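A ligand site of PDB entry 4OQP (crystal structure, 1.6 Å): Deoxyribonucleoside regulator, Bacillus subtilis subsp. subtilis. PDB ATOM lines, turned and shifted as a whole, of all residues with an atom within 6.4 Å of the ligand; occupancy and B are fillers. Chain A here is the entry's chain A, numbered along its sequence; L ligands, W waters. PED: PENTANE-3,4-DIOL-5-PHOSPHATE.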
ATOM      1  N   TYR A  38      -5.291  -7.310  -9.851  1.00  0.00           N
ATOM      2  CA  TYR A  38      -6.195  -8.422  -9.741  1.00  0.00           C
ATOM      3  C   TYR A  38      -5.489  -9.790  -9.650  1.00  0.00           C
ATOM      4  O   TYR A  38      -5.884 -10.630  -8.852  1.00  0.00           O
ATOM      5  CB  TYR A  38      -7.205  -8.409 -10.913  1.00  0.00           C
ATOM      6  CG  TYR A  38      -8.226  -9.511 -10.832  1.00  0.00           C
ATOM      7  CD1 TYR A  38      -9.355  -9.379 -10.027  1.00  0.00           C
ATOM      8  CD2 TYR A  38      -8.088 -10.691 -11.565  1.00  0.00           C
ATOM      9  CE1 TYR A  38     -10.293 -10.371  -9.919  1.00  0.00           C
ATOM     10  CE2 TYR A  38      -9.029 -11.705 -11.453  1.00  0.00           C
ATOM     11  CZ  TYR A  38     -10.144 -11.534 -10.644  1.00  0.00           C
ATOM     12  OH  TYR A  38     -11.044 -12.550 -10.536  1.00  0.00           O
ATOM     13  N   SER A  66     -18.213 -24.463  -6.569  1.00  0.00           N
ATOM     14  CA  SER A  66     -18.492 -23.703  -7.783  1.00  0.00           C
ATOM     15  C   SER A  66     -17.352 -23.995  -8.814  1.00  0.00           C
ATOM     16  O   SER A  66     -16.575 -24.968  -8.696  1.00  0.00           O
ATOM     17  CB  SER A  66     -18.566 -22.207  -7.398  1.00  0.00           C
ATOM     18  OG  SER A  66     -19.014 -21.355  -8.488  1.00  0.00           O
ATOM     19  N   TRP A  67     -17.230 -23.123  -9.801  1.00  0.00           N
ATOM     20  CA  TRP A  67     -16.136 -23.199 -10.733  1.00  0.00           C
ATOM     21  C   TRP A  67     -15.758 -21.824 -11.256  1.00  0.00           C
ATOM     22  O   TRP A  67     -16.330 -20.807 -10.844  1.00  0.00           O
ATOM     23  CB  TRP A  67     -16.442 -24.178 -11.871  1.00  0.00           C
ATOM     24  CG  TRP A  67     -17.774 -24.026 -12.595  1.00  0.00           C
ATOM     25  CD1 TRP A  67     -18.844 -24.852 -12.472  1.00  0.00           C
ATOM     26  CD2 TRP A  67     -18.118 -23.082 -13.606  1.00  0.00           C
ATOM     27  NE1 TRP A  67     -19.852 -24.446 -13.291  1.00  0.00           N
ATOM     28  CE2 TRP A  67     -19.457 -23.347 -13.979  1.00  0.00           C
ATOM     29  CE3 TRP A  67     -17.486 -21.947 -14.142  1.00  0.00           C
ATOM     30  CZ2 TRP A  67     -20.125 -22.590 -14.905  1.00  0.00           C
ATOM     31  CZ3 TRP A  67     -18.161 -21.193 -15.092  1.00  0.00           C
ATOM     32  CH2 TRP A  67     -19.482 -21.520 -15.438  1.00  0.00           C
ATOM     33  N   GLY A  68     -14.708 -21.807 -12.073  1.00  0.00           N
ATOM     34  CA  GLY A  68     -14.200 -20.592 -12.661  1.00  0.00           C
ATOM     35  C   GLY A  68     -12.735 -20.380 -12.291  1.00  0.00           C
ATOM     36  O   GLY A  68     -12.131 -21.231 -11.713  1.00  0.00           O
ATOM     37  N   THR A  69     -12.194 -19.223 -12.605  1.00  0.00           N
ATOM     38  CA  THR A  69     -10.732 -19.037 -12.519  1.00  0.00           C
ATOM     39  C   THR A  69     -10.278 -19.007 -11.056  1.00  0.00           C
ATOM     40  O   THR A  69      -9.223 -19.579 -10.723  1.00  0.00           O
ATOM     41  CB  THR A  69     -10.241 -17.812 -13.331  1.00  0.00           C
ATOM     42  OG1 THR A  69     -10.827 -16.604 -12.854  1.00  0.00           O
ATOM     43  CG2 THR A  69     -10.550 -17.996 -14.813  1.00  0.00           C
ATOM     44  N   THR A  70     -11.037 -18.349 -10.193  1.00  0.00           N
ATOM     45  CA  THR A  70     -10.725 -18.348  -8.766  1.00  0.00           C
ATOM     46  C   THR A  70     -10.793 -19.756  -8.163  1.00  0.00           C
ATOM     47  O   THR A  70      -9.908 -20.201  -7.452  1.00  0.00           O
ATOM     48  CB  THR A  70     -11.694 -17.387  -7.999  1.00  0.00           C
ATOM     49  OG1 THR A  70     -11.737 -16.124  -8.677  1.00  0.00           O
ATOM     50  CG2 THR A  70     -11.276 -17.216  -6.575  1.00  0.00           C
ATOM     51  N   MET A  71     -11.900 -20.444  -8.430  1.00  0.00           N
ATOM     52  CA  MET A  71     -12.091 -21.762  -7.876  1.00  0.00           C
ATOM     53  C   MET A  71     -10.999 -22.759  -8.333  1.00  0.00           C
ATOM     54  O   MET A  71     -10.552 -23.583  -7.564  1.00  0.00           O
ATOM     55  CB  MET A  71     -13.499 -22.282  -8.222  1.00  0.00           C
ATOM     56  CG  MET A  71     -14.609 -21.503  -7.569  1.00  0.00           C
ATOM     57  SD  MET A  71     -14.674 -21.717  -5.789  1.00  0.00           S
ATOM     58  CE  MET A  71     -14.894 -23.483  -5.737  1.00  0.00           C
ATOM     59  N   LYS A  92     -23.165 -26.316  -9.616  1.00  0.00           N
ATOM     60  CA  LYS A  92     -23.749 -25.926 -10.902  1.00  0.00           C
ATOM     61  C   LYS A  92     -22.946 -26.644 -11.987  1.00  0.00           C
ATOM     62  O   LYS A  92     -21.742 -26.845 -11.833  1.00  0.00           O
ATOM     63  CB  LYS A  92     -23.678 -24.419 -11.156  1.00  0.00           C
ATOM     64  CG  LYS A  92     -22.342 -23.788 -10.907  1.00  0.00           C
ATOM     65  CD  LYS A  92     -22.162 -22.460 -11.587  1.00  0.00           C
ATOM     66  CE  LYS A  92     -20.834 -21.877 -11.119  1.00  0.00           C
ATOM     67  NZ  LYS A  92     -20.580 -20.536 -11.665  1.00  0.00           N
ATOM     68  N   PHE A 158     -17.584 -20.641  -3.208  1.00  0.00           N
ATOM     69  CA  PHE A 158     -17.784 -19.930  -4.453  1.00  0.00           C
ATOM     70  C   PHE A 158     -17.150 -18.563  -4.495  1.00  0.00           C
ATOM     71  O   PHE A 158     -16.643 -18.051  -3.503  1.00  0.00           O
ATOM     72  CB  PHE A 158     -19.302 -19.817  -4.703  1.00  0.00           C
ATOM     73  CG  PHE A 158     -20.050 -19.211  -3.547  1.00  0.00           C
ATOM     74  CD1 PHE A 158     -20.163 -17.837  -3.429  1.00  0.00           C
ATOM     75  CD2 PHE A 158     -20.599 -20.002  -2.561  1.00  0.00           C
ATOM     76  CE1 PHE A 158     -20.823 -17.267  -2.352  1.00  0.00           C
ATOM     77  CE2 PHE A 158     -21.262 -19.453  -1.480  1.00  0.00           C
ATOM     78  CZ  PHE A 158     -21.365 -18.081  -1.362  1.00  0.00           C
ATOM     79  N   THR A 159     -17.127 -17.986  -5.717  1.00  0.00           N
ATOM     80  CA  THR A 159     -16.719 -16.627  -5.900  1.00  0.00           C
ATOM     81  C   THR A 159     -17.917 -15.846  -6.387  1.00  0.00           C
ATOM     82  O   THR A 159     -19.032 -16.386  -6.388  1.00  0.00           O
ATOM     83  CB  THR A 159     -15.562 -16.484  -6.913  1.00  0.00           C
ATOM     84  OG1 THR A 159     -14.995 -15.170  -6.835  1.00  0.00           O
ATOM     85  CG2 THR A 159     -16.006 -16.728  -8.301  1.00  0.00           C
ATOM     86  N   VAL A 160     -17.712 -14.568  -6.653  1.00  0.00           N
ATOM     87  CA  VAL A 160     -18.722 -13.797  -7.395  1.00  0.00           C
ATOM     88  C   VAL A 160     -18.078 -13.339  -8.718  1.00  0.00           C
ATOM     89  O   VAL A 160     -16.895 -12.940  -8.757  1.00  0.00           O
ATOM     90  CB  VAL A 160     -19.347 -12.662  -6.512  1.00  0.00           C
ATOM     91  CG1 VAL A 160     -18.302 -11.729  -5.939  1.00  0.00           C
ATOM     92  CG2 VAL A 160     -20.410 -11.858  -7.275  1.00  0.00           C
ATOM     93  N   GLY A 161     -18.855 -13.387  -9.801  1.00  0.00           N
ATOM     94  CA  GLY A 161     -18.356 -12.995 -11.106  1.00  0.00           C
ATOM     95  C   GLY A 161     -18.706 -11.544 -11.392  1.00  0.00           C
ATOM     96  O   GLY A 161     -19.338 -10.904 -10.575  1.00  0.00           O
ATOM     97  N   THR A 162     -18.218 -11.018 -12.490  1.00  0.00           N
ATOM     98  CA  THR A 162     -18.455  -9.639 -12.914  1.00  0.00           C
ATOM     99  C   THR A 162     -19.395  -9.655 -14.114  1.00  0.00           C
ATOM    100  O   THR A 162     -19.870 -10.699 -14.571  1.00  0.00           O
ATOM    101  CB  THR A 162     -17.139  -8.946 -13.382  1.00  0.00           C
ATOM    102  OG1 THR A 162     -16.781  -9.477 -14.663  1.00  0.00           O
ATOM    103  CG2 THR A 162     -16.035  -9.133 -12.319  1.00  0.00           C
ATOM    104  N   ALA A 167     -16.083 -11.540 -19.166  1.00  0.00           N
ATOM    105  CA  ALA A 167     -16.630 -12.420 -18.133  1.00  0.00           C
ATOM    106  C   ALA A 167     -16.800 -13.845 -18.669  1.00  0.00           C
ATOM    107  O   ALA A 167     -17.281 -14.062 -19.769  1.00  0.00           O
ATOM    108  CB  ALA A 167     -17.959 -11.870 -17.591  1.00  0.00           C
ATOM    109  N   LEU A 168     -16.321 -14.817 -17.907  1.00  0.00           N
ATOM    110  CA  LEU A 168     -16.416 -16.188 -18.338  1.00  0.00           C
ATOM    111  C   LEU A 168     -17.836 -16.601 -18.782  1.00  0.00           C
ATOM    112  O   LEU A 168     -18.032 -17.297 -19.782  1.00  0.00           O
ATOM    113  CB  LEU A 168     -15.886 -17.070 -17.210  1.00  0.00           C
ATOM    114  CG  LEU A 168     -15.794 -18.557 -17.430  1.00  0.00           C
ATOM    115  CD1 LEU A 168     -15.006 -18.911 -18.694  1.00  0.00           C
ATOM    116  CD2 LEU A 168     -15.169 -19.228 -16.199  1.00  0.00           C
ATOM    117  N   LEU A 169     -18.845 -16.177 -18.037  1.00  0.00           N
ATOM    118  CA  LEU A 169     -20.230 -16.562 -18.349  1.00  0.00           C
ATOM    119  C   LEU A 169     -20.776 -15.957 -19.627  1.00  0.00           C
ATOM    120  O   LEU A 169     -21.841 -16.341 -20.101  1.00  0.00           O
ATOM    121  CB  LEU A 169     -21.142 -16.250 -17.184  1.00  0.00           C
ATOM    122  CG  LEU A 169     -21.221 -17.312 -16.108  1.00  0.00           C
ATOM    123  CD1 LEU A 169     -22.028 -16.756 -14.945  1.00  0.00           C
ATOM    124  CD2 LEU A 169     -21.856 -18.609 -16.618  1.00  0.00           C
ATOM    125  N   ASP A 190     -22.573 -12.375 -10.553  1.00  0.00           N
ATOM    126  CA  ASP A 190     -23.262 -13.672 -10.415  1.00  0.00           C
ATOM    127  C   ASP A 190     -22.659 -14.417  -9.243  1.00  0.00           C
ATOM    128  O   ASP A 190     -21.486 -14.236  -8.926  1.00  0.00           O
ATOM    129  CB  ASP A 190     -23.126 -14.545 -11.683  1.00  0.00           C
ATOM    130  CG  ASP A 190     -21.775 -15.239 -11.745  1.00  0.00           C
ATOM    131  OD1 ASP A 190     -20.865 -14.564 -12.241  1.00  0.00           O
ATOM    132  OD2 ASP A 190     -21.647 -16.417 -11.291  1.00  0.00           O
ATOM    133  N   ILE A 191     -23.445 -15.258  -8.562  1.00  0.00           N
ATOM    134  CA  ILE A 191     -22.971 -16.321  -7.711  1.00  0.00           C
ATOM    135  C   ILE A 191     -23.508 -17.580  -8.298  1.00  0.00           C
ATOM    136  O   ILE A 191     -24.721 -17.702  -8.561  1.00  0.00           O
ATOM    137  CB  ILE A 191     -23.411 -16.189  -6.247  1.00  0.00           C
ATOM    138  CG1 ILE A 191     -22.618 -15.053  -5.575  1.00  0.00           C
ATOM    139  CG2 ILE A 191     -23.174 -17.507  -5.485  1.00  0.00           C
ATOM    140  CD1 ILE A 191     -23.189 -14.620  -4.257  1.00  0.00           C
ATOM    141  N   CYS A 192     -22.636 -18.541  -8.541  1.00  0.00           N
ATOM    142  CA  CYS A 192     -23.054 -19.790  -9.165  1.00  0.00           C
ATOM    143  C   CYS A 192     -23.917 -19.517 -10.402  1.00  0.00           C
ATOM    144  O   CYS A 192     -24.919 -20.248 -10.661  1.00  0.00           O
ATOM    145  CB  CYS A 192     -23.736 -20.744  -8.191  1.00  0.00           C
ATOM    146  SG  CYS A 192     -22.533 -21.332  -6.923  1.00  0.00           S
ATOM    147  N   SER A 193     -23.502 -18.523 -11.191  1.00  0.00           N
ATOM    148  CA  SER A 193     -24.102 -18.263 -12.499  1.00  0.00           C
ATOM    149  C   SER A 193     -25.537 -17.739 -12.440  1.00  0.00           C
ATOM    150  O   SER A 193     -26.200 -17.636 -13.467  1.00  0.00           O
ATOM    151  CB  SER A 193     -23.969 -19.432 -13.463  1.00  0.00           C
ATOM    152  OG  SER A 193     -22.606 -19.711 -13.706  1.00  0.00           O
ATOM    153  N   LYS A 234     -14.316  -6.409  -8.798  1.00  0.00           N
ATOM    154  CA  LYS A 234     -15.330  -7.157  -8.078  1.00  0.00           C
ATOM    155  C   LYS A 234     -15.934  -6.421  -6.876  1.00  0.00           C
ATOM    156  O   LYS A 234     -16.759  -6.994  -6.164  1.00  0.00           O
ATOM    157  CB  LYS A 234     -14.756  -8.529  -7.642  1.00  0.00           C
ATOM    158  CG  LYS A 234     -14.521  -9.513  -8.786  1.00  0.00           C
ATOM    159  CD  LYS A 234     -14.289 -10.933  -8.364  1.00  0.00           C
ATOM    160  CE  LYS A 234     -14.240 -11.841  -9.563  1.00  0.00           C
ATOM    161  NZ  LYS A 234     -14.219 -13.280  -9.250  1.00  0.00           N
HETATM  162  P   PED L   1     -14.069 -16.181 -11.763  1.00  0.00           P
HETATM  163  O1P PED L   1     -14.433 -14.783 -11.579  1.00  0.00           O
HETATM  164  O2P PED L   1     -13.415 -16.783 -10.591  1.00  0.00           O
HETATM  165  O3P PED L   1     -13.507 -16.504 -13.124  1.00  0.00           O
HETATM  166  O5' PED L   1     -15.508 -16.998 -11.759  1.00  0.00           O
HETATM  167  C2' PED L   1     -19.170 -18.656 -12.415  1.00  0.00           C
HETATM  168  C5' PED L   1     -16.463 -16.706 -12.699  1.00  0.00           C
HETATM  169  C4' PED L   1     -17.826 -16.531 -11.999  1.00  0.00           C
HETATM  170  O4' PED L   1     -18.688 -15.955 -13.027  1.00  0.00           O
HETATM  171  C3' PED L   1     -18.427 -17.807 -11.393  1.00  0.00           C
HETATM  172  C1' PED L   1     -19.421 -20.000 -11.827  1.00  0.00           C
HETATM  173  O3' PED L   1     -19.366 -17.345 -10.390  1.00  0.00           O
HETATM  174  O   HOH W   1     -14.397 -14.558 -15.537  1.00  0.00           O
HETATM  175  O   HOH W   2     -18.376 -14.729 -15.411  1.00  0.00           O
HETATM  176  O   HOH W   3     -14.235 -19.226  -9.731  1.00  0.00           O
HETATM  177  O   HOH W   4     -19.751 -18.451  -8.100  1.00  0.00           O
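The side-chain hydroxyl of Thr 70 sits at hydrogen-bond distance from an oxygen (O2P) of the ligand (2.6 Å).
O3P of the ligand lies within hydrogen-bond range of OG1 of Thr 69.
The side-chain amino group (NZ) of Lys 92 is bonded to a carbon (C1') of the ligand (1.3 Å).
An oxygen (O1P) of the ligand is in salt-bridge range of the side-chain amino group of Lys 234 (2.8 Å).
The side-chain carboxylate (OD2) of Asp 190 lies within hydrogen-bond range of an oxygen (O3') of the ligand (2.6 Å).
An oxygen (O2P) of the ligand sits at hydrogen-bond distance from the backbone NH of Thr 70, at 2.9 Å.
The backbone NH (N) of Thr 69 is in hydrogen-bond range of an oxygen (O3P) of the ligand (3.1 Å).
The side-chain carboxylate (OD2) of Asp 190 is in hydrogen-bond range of the backbone NH (N) of Ser 193 (2.8 Å).
NE1 of Trp 67 lies within hydrogen-bond range of O of Lys 92, 3.4 Å away.
NZ of Lys 234 lies within hydrogen-bond range of O of Val 160 (2.7 Å).
The side-chain amino group (NZ) of Lys 92 sits at hydrogen-bond distance from the side-chain hydroxyl (OG) of Ser 193 (3.0 Å).
O of Asp 190 sits at hydrogen-bond distance from N of Gly 161, 2.9 Å away.
NZ of Lys 234 is in hydrogen-bond range of OG1 of Thr 159 (3.2 Å).
Merely in contact with the ligand: Ser 66 (3.6 Å), Trp 67 (3.3 Å), Gly 68 (3.9 Å), Thr 159 (3.5 Å), Gly 161 (3.5 Å), Leu 169 (3.9 Å), Cys 192 (3.9 Å) and Ser 193 (3.7 Å).
Hydrophobic or aromatic side chains within 4 Å of the ligand: Trp 67 and Leu 169.
Within 4 Å of the ligand: Ser 66, Trp 67, Gly 68, Thr 69, Thr 70, Lys 92, Thr 159, Gly 161, Leu 169, Asp 190, Cys 192, Ser 193 and Lys 234.
Water W4 lies within hydrogen-bond range of O3' of the ligand, O of Thr 159, N of Cys 192 and OG of Ser 66.
Water W2 lies within hydrogen-bond range of an oxygen (O4') of the ligand, the backbone NH (N) of Leu 169 and the backbone NH (N) of Leu 168.
Water W3 lies within hydrogen-bond range of an oxygen (O2P) of the ligand (2.7 Å), the backbone carbonyl oxygen of Trp 67 (2.9 Å), the backbone NH of Met 71 (2.9 Å) and the backbone NH of Thr 70 (3.3 Å).
Water W1 bridges the backbone NH of Leu 168 and an oxygen (O3P) of the ligand.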
